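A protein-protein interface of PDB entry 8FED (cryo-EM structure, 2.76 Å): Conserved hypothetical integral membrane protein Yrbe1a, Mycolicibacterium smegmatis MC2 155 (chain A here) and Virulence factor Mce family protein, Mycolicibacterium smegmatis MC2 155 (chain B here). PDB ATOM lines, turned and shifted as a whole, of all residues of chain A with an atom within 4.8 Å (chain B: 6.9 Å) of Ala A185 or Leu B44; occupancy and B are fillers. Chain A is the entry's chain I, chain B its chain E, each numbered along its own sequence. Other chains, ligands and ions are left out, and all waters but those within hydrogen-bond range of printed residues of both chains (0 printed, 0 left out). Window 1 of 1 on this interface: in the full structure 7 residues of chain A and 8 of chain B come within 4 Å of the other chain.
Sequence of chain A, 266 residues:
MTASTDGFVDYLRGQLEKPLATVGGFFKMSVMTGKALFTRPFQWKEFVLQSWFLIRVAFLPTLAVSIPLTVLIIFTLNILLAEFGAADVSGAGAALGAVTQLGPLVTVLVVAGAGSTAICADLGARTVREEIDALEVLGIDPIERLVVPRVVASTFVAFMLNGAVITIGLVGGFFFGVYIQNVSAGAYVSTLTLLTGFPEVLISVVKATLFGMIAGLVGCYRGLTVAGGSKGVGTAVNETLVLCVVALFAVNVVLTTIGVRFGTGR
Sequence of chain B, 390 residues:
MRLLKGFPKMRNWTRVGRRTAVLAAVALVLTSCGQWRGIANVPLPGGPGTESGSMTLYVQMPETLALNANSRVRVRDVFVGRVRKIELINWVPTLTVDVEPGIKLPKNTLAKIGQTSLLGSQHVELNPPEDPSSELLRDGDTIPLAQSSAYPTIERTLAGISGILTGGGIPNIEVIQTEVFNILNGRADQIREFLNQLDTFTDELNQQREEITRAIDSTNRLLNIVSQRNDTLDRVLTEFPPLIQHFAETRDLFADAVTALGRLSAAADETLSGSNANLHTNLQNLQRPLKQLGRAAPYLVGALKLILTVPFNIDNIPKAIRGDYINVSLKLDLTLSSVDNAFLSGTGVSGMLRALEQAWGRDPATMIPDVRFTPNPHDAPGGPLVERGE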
ATOM      1  N   PHE A 174       7.457 -13.413   2.130  1.00  0.00           N
ATOM      2  CA  PHE A 174       6.412 -12.445   1.811  1.00  0.00           C
ATOM      3  C   PHE A 174       5.430 -13.021   0.802  1.00  0.00           C
ATOM      4  O   PHE A 174       4.211 -13.000   1.022  1.00  0.00           O
ATOM      5  CB  PHE A 174       7.037 -11.157   1.271  1.00  0.00           C
ATOM      6  CG  PHE A 174       6.047 -10.216   0.637  1.00  0.00           C
ATOM      7  CD1 PHE A 174       5.319  -9.334   1.416  1.00  0.00           C
ATOM      8  CD2 PHE A 174       5.860 -10.196  -0.737  1.00  0.00           C
ATOM      9  CE1 PHE A 174       4.415  -8.466   0.841  1.00  0.00           C
ATOM     10  CE2 PHE A 174       4.953  -9.331  -1.315  1.00  0.00           C
ATOM     11  CZ  PHE A 174       4.231  -8.465  -0.526  1.00  0.00           C
ATOM     12  N   VAL A 178       1.524 -14.018   1.683  1.00  0.00           N
ATOM     13  CA  VAL A 178       0.474 -13.183   1.112  1.00  0.00           C
ATOM     14  C   VAL A 178      -0.411 -13.989   0.168  1.00  0.00           C
ATOM     15  O   VAL A 178      -1.639 -13.995   0.303  1.00  0.00           O
ATOM     16  CB  VAL A 178       1.087 -11.958   0.411  1.00  0.00           C
ATOM     17  CG1 VAL A 178       0.045 -11.256  -0.442  1.00  0.00           C
ATOM     18  CG2 VAL A 178       1.660 -11.004   1.442  1.00  0.00           C
ATOM     19  N   VAL A 183      -2.375 -13.574   4.440  1.00  0.00           N
ATOM     20  CA  VAL A 183      -2.087 -12.555   5.443  1.00  0.00           C
ATOM     21  C   VAL A 183      -1.975 -11.215   4.730  1.00  0.00           C
ATOM     22  O   VAL A 183      -1.891 -11.161   3.498  1.00  0.00           O
ATOM     23  CB  VAL A 183      -0.810 -12.873   6.242  1.00  0.00           C
ATOM     24  CG1 VAL A 183      -0.881 -14.273   6.824  1.00  0.00           C
ATOM     25  CG2 VAL A 183       0.424 -12.703   5.374  1.00  0.00           C
ATOM     26  N   SER A 184      -1.982 -10.127   5.491  1.00  0.00           N
ATOM     27  CA  SER A 184      -1.902  -8.796   4.907  1.00  0.00           C
ATOM     28  C   SER A 184      -0.450  -8.441   4.606  1.00  0.00           C
ATOM     29  O   SER A 184       0.426  -8.576   5.466  1.00  0.00           O
ATOM     30  CB  SER A 184      -2.546  -7.764   5.829  1.00  0.00           C
ATOM     31  OG  SER A 184      -1.854  -7.663   7.050  1.00  0.00           O
ATOM     32  N   ALA A 185      -0.206  -7.992   3.372  1.00  0.00           N
ATOM     33  CA  ALA A 185       1.138  -7.621   2.939  1.00  0.00           C
ATOM     34  C   ALA A 185       1.691  -6.441   3.731  1.00  0.00           C
ATOM     35  O   ALA A 185       2.882  -6.418   4.075  1.00  0.00           O
ATOM     36  CB  ALA A 185       1.127  -7.300   1.446  1.00  0.00           C
ATOM     37  N   GLY A 186       0.850  -5.445   4.009  1.00  0.00           N
ATOM     38  CA  GLY A 186       1.301  -4.302   4.786  1.00  0.00           C
ATOM     39  C   GLY A 186       1.771  -4.673   6.179  1.00  0.00           C
ATOM     40  O   GLY A 186       2.708  -4.071   6.703  1.00  0.00           O
ATOM     41  N   ALA A 187       1.128  -5.662   6.802  1.00  0.00           N
ATOM     42  CA  ALA A 187       1.606  -6.120   8.101  1.00  0.00           C
ATOM     43  C   ALA A 187       2.936  -6.846   7.991  1.00  0.00           C
ATOM     44  O   ALA A 187       3.740  -6.802   8.928  1.00  0.00           O
ATOM     45  CB  ALA A 187       0.578  -7.021   8.778  1.00  0.00           C
ATOM     46  N   TYR A 188       3.180  -7.531   6.874  1.00  0.00           N
ATOM     47  CA  TYR A 188       4.463  -8.200   6.702  1.00  0.00           C
ATOM     48  C   TYR A 188       5.588  -7.190   6.513  1.00  0.00           C
ATOM     49  O   TYR A 188       6.625  -7.275   7.177  1.00  0.00           O
ATOM     50  CB  TYR A 188       4.405  -9.172   5.522  1.00  0.00           C
ATOM     51  CG  TYR A 188       5.637 -10.042   5.399  1.00  0.00           C
ATOM     52  CD1 TYR A 188       6.734  -9.635   4.648  1.00  0.00           C
ATOM     53  CD2 TYR A 188       5.706 -11.269   6.042  1.00  0.00           C
ATOM     54  CE1 TYR A 188       7.860 -10.426   4.545  1.00  0.00           C
ATOM     55  CE2 TYR A 188       6.827 -12.068   5.939  1.00  0.00           C
ATOM     56  CZ  TYR A 188       7.900 -11.641   5.188  1.00  0.00           C
ATOM     57  OH  TYR A 188       9.021 -12.432   5.085  1.00  0.00           O
ATOM     58  N   VAL A 189       5.396  -6.216   5.621  1.00  0.00           N
ATOM     59  CA  VAL A 189       6.510  -5.327   5.296  1.00  0.00           C
ATOM     60  C   VAL A 189       6.749  -4.281   6.383  1.00  0.00           C
ATOM     61  O   VAL A 189       7.889  -3.851   6.588  1.00  0.00           O
ATOM     62  CB  VAL A 189       6.296  -4.664   3.925  1.00  0.00           C
ATOM     63  CG1 VAL A 189       6.368  -5.703   2.823  1.00  0.00           C
ATOM     64  CG2 VAL A 189       4.971  -3.925   3.883  1.00  0.00           C
ATOM     65  N   ILE B  39      10.873   0.467   3.330  1.00  0.00           N
ATOM     66  CA  ILE B  39      10.267  -0.753   2.804  1.00  0.00           C
ATOM     67  C   ILE B  39       8.783  -0.814   3.150  1.00  0.00           C
ATOM     68  O   ILE B  39       7.993  -1.430   2.426  1.00  0.00           O
ATOM     69  CB  ILE B  39      11.037  -1.985   3.324  1.00  0.00           C
ATOM     70  CG1 ILE B  39      10.536  -3.267   2.658  1.00  0.00           C
ATOM     71  CG2 ILE B  39      10.943  -2.087   4.841  1.00  0.00           C
ATOM     72  CD1 ILE B  39      10.696  -3.273   1.158  1.00  0.00           C
ATOM     73  N   ALA B  40       8.374  -0.176   4.247  1.00  0.00           N
ATOM     74  CA  ALA B  40       6.973  -0.188   4.643  1.00  0.00           C
ATOM     75  C   ALA B  40       6.105   0.723   3.787  1.00  0.00           C
ATOM     76  O   ALA B  40       4.883   0.544   3.766  1.00  0.00           O
ATOM     77  CB  ALA B  40       6.843   0.215   6.113  1.00  0.00           C
ATOM     78  N   VAL B  42       6.493   1.384   0.348  1.00  0.00           N
ATOM     79  CA  VAL B  42       6.563   1.147  -1.093  1.00  0.00           C
ATOM     80  C   VAL B  42       5.323   0.365  -1.513  1.00  0.00           C
ATOM     81  O   VAL B  42       4.889  -0.542  -0.786  1.00  0.00           O
ATOM     82  CB  VAL B  42       7.870   0.427  -1.475  1.00  0.00           C
ATOM     83  CG1 VAL B  42       8.027  -0.875  -0.712  1.00  0.00           C
ATOM     84  CG2 VAL B  42       7.945   0.177  -2.974  1.00  0.00           C
ATOM     85  N   PRO B  43       4.685   0.713  -2.634  1.00  0.00           N
ATOM     86  CA  PRO B  43       3.530  -0.065  -3.098  1.00  0.00           C
ATOM     87  C   PRO B  43       3.905  -1.511  -3.388  1.00  0.00           C
ATOM     88  O   PRO B  43       5.009  -1.811  -3.846  1.00  0.00           O
ATOM     89  CB  PRO B  43       3.097   0.669  -4.372  1.00  0.00           C
ATOM     90  CG  PRO B  43       3.590   2.059  -4.185  1.00  0.00           C
ATOM     91  CD  PRO B  43       4.881   1.936  -3.433  1.00  0.00           C
ATOM     92  N   LEU B  44       2.964  -2.412  -3.116  1.00  0.00           N
ATOM     93  CA  LEU B  44       3.195  -3.836  -3.273  1.00  0.00           C
ATOM     94  C   LEU B  44       2.203  -4.434  -4.263  1.00  0.00           C
ATOM     95  O   LEU B  44       1.062  -3.976  -4.359  1.00  0.00           O
ATOM     96  CB  LEU B  44       3.071  -4.557  -1.926  1.00  0.00           C
ATOM     97  CG  LEU B  44       4.031  -4.089  -0.833  1.00  0.00           C
ATOM     98  CD1 LEU B  44       3.710  -4.771   0.479  1.00  0.00           C
ATOM     99  CD2 LEU B  44       5.470  -4.349  -1.236  1.00  0.00           C
ATOM    100  N   PRO B  45       2.610  -5.453  -5.015  1.00  0.00           N
ATOM    101  CA  PRO B  45       1.708  -6.053  -5.999  1.00  0.00           C
ATOM    102  C   PRO B  45       0.677  -6.965  -5.350  1.00  0.00           C
ATOM    103  O   PRO B  45       0.849  -7.465  -4.239  1.00  0.00           O
ATOM    104  CB  PRO B  45       2.656  -6.852  -6.900  1.00  0.00           C
ATOM    105  CG  PRO B  45       3.772  -7.230  -5.993  1.00  0.00           C
ATOM    106  CD  PRO B  45       3.945  -6.077  -5.038  1.00  0.00           C
ATOM    107  N   GLY B  46      -0.419  -7.169  -6.077  1.00  0.00           N
ATOM    108  CA  GLY B  46      -1.455  -8.088  -5.660  1.00  0.00           C
ATOM    109  C   GLY B  46      -2.394  -7.493  -4.629  1.00  0.00           C
ATOM    110  O   GLY B  46      -2.146  -6.444  -4.032  1.00  0.00           O
ATOM    111  N   GLY B  47      -3.500  -8.198  -4.409  1.00  0.00           N
ATOM    112  CA  GLY B  47      -4.501  -7.773  -3.463  1.00  0.00           C
ATOM    113  C   GLY B  47      -5.600  -6.963  -4.117  1.00  0.00           C
ATOM    114  O   GLY B  47      -5.469  -6.506  -5.256  1.00  0.00           O
ATOM    115  N   THR B  50      -5.717  -3.607  -6.823  1.00  0.00           N
ATOM    116  CA  THR B  50      -4.541  -3.603  -7.679  1.00  0.00           C
ATOM    117  C   THR B  50      -4.813  -4.150  -9.073  1.00  0.00           C
ATOM    118  O   THR B  50      -3.985  -3.951  -9.970  1.00  0.00           O
ATOM    119  CB  THR B  50      -3.410  -4.407  -7.030  1.00  0.00           C
ATOM    120  OG1 THR B  50      -3.843  -5.756  -6.817  1.00  0.00           O
ATOM    121  CG2 THR B  50      -3.022  -3.790  -5.698  1.00  0.00           C
ATOM    122  N   ALA B  69       1.863   3.154   4.180  1.00  0.00           N
ATOM    123  CA  ALA B  69       1.287   2.758   2.906  1.00  0.00           C
ATOM    124  C   ALA B  69       0.977   1.262   2.916  1.00  0.00           C
ATOM    125  O   ALA B  69       1.375   0.521   3.820  1.00  0.00           O
ATOM    126  CB  ALA B  69       2.229   3.106   1.755  1.00  0.00           C
ATOM    127  N   ASN B  70       0.231   0.827   1.899  1.00  0.00           N
ATOM    128  CA  ASN B  70      -0.240  -0.546   1.722  1.00  0.00           C
ATOM    129  C   ASN B  70      -1.217  -0.983   2.806  1.00  0.00           C
ATOM    130  O   ASN B  70      -1.565  -2.168   2.871  1.00  0.00           O
ATOM    131  CB  ASN B  70       0.916  -1.552   1.647  1.00  0.00           C
ATOM    132  CG  ASN B  70       1.898  -1.224   0.548  1.00  0.00           C
ATOM    133  OD1 ASN B  70       1.509  -0.950  -0.585  1.00  0.00           O
ATOM    134  ND2 ASN B  70       3.183  -1.238   0.879  1.00  0.00           N
ATOM    135  N   ARG B  72      -4.936  -1.213   4.797  1.00  0.00           N
ATOM    136  CA  ARG B  72      -6.189  -1.744   4.282  1.00  0.00           C
ATOM    137  C   ARG B  72      -7.265  -0.667   4.235  1.00  0.00           C
ATOM    138  O   ARG B  72      -7.430   0.105   5.186  1.00  0.00           O
ATOM    139  CB  ARG B  72      -6.661  -2.919   5.137  1.00  0.00           C
ATOM    140  CG  ARG B  72      -5.720  -4.113   5.134  1.00  0.00           C
ATOM    141  CD  ARG B  72      -6.399  -5.330   5.739  1.00  0.00           C
ATOM    142  NE  ARG B  72      -5.780  -6.581   5.320  1.00  0.00           N
ATOM    143  CZ  ARG B  72      -6.193  -7.782   5.701  1.00  0.00           C
ATOM    144  NH1 ARG B  72      -7.217  -7.929   6.524  1.00  0.00           N
ATOM    145  NH2 ARG B  72      -5.571  -8.861   5.238  1.00  0.00           N
ATOM    146  N   ARG B  82      -6.703  -0.677  -0.992  1.00  0.00           N
ATOM    147  CA  ARG B  82      -5.365  -0.420  -0.483  1.00  0.00           C
ATOM    148  C   ARG B  82      -5.047   1.061  -0.635  1.00  0.00           C
ATOM    149  O   ARG B  82      -5.476   1.704  -1.596  1.00  0.00           O
ATOM    150  CB  ARG B  82      -4.323  -1.267  -1.232  1.00  0.00           C
ATOM    151  CG  ARG B  82      -2.880  -1.035  -0.817  1.00  0.00           C
ATOM    152  CD  ARG B  82      -1.917  -1.444  -1.916  1.00  0.00           C
ATOM    153  NE  ARG B  82      -2.171  -0.715  -3.153  1.00  0.00           N
ATOM    154  CZ  ARG B  82      -1.450  -0.837  -4.258  1.00  0.00           C
ATOM    155  NH1 ARG B  82      -0.410  -1.653  -4.318  1.00  0.00           N
ATOM    156  NH2 ARG B  82      -1.780  -0.124  -5.330  1.00  0.00           N
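The backbone NH (N) of Leu B44 is in hydrogen-bond range of the side-chain amide oxygen (OD1) of Asn B70. The backbone carbonyl oxygen (O) of Leu B44 is in hydrogen-bond range of the guanidinium group (NH1) of Arg B82 (2.8 Å). The backbone NH (N) of Phe A174 sits at hydrogen-bond distance from the side-chain hydroxyl (OH) of Tyr A188 (3.5 Å).
Among the printed residues, pairs that only touch across the chains: Ser A184 with Arg B72 (3.3 Å), Val A189 with Leu B44 (3.7 Å), Ala A185 with Leu B44 (3.7 Å), Phe A174 with Leu B44 (3.8 Å) and Val A189 with Ile B39 (3.9 Å).
Val A178 touches none of the printed residues of chain B. Printed residues of chain B within 4 Å of Ser A184: Arg B72 (3.3 Å). Ala A185 touches just one residue of chain B: Leu B44 (3.7 Å). Of the printed residues of chain B, Val A189 touches Ile B39 (3.9 Å) and Leu B44 (3.7 Å). Of the printed residues of chain A, Ile B39 touches Val A189. Of chain A, only Phe A174 (3.8 Å), Ala A185 (3.7 Å) and Val A189 (3.7 Å) come within 4 Å of Leu B44. Of the printed residues of chain A, Arg B72 touches Ser A184 (3.3 Å). Arg B82 touches none of the printed residues of chain A. The nearest residue of chain A that does not touch Leu B44 is Gly A186 (4.6 Å). The nearest printed residue of chain B that does not touch Ser A184 is Asn B70 (6.4 Å).
Of the 13 printed residues of chain B, 3 touch a printed residue of chain A. Printed residues of chain B that touch a printed residue of chain A: Ile B39, Leu B44 and Arg B72. Hydrophobic or aromatic side chains of chain B within 4 Å of the printed part of chain A: Ile B39 and Leu B44. Printed residues of chain A that touch a printed residue of chain B: Phe A174, Ser A184, Ala A185 and Val A189.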
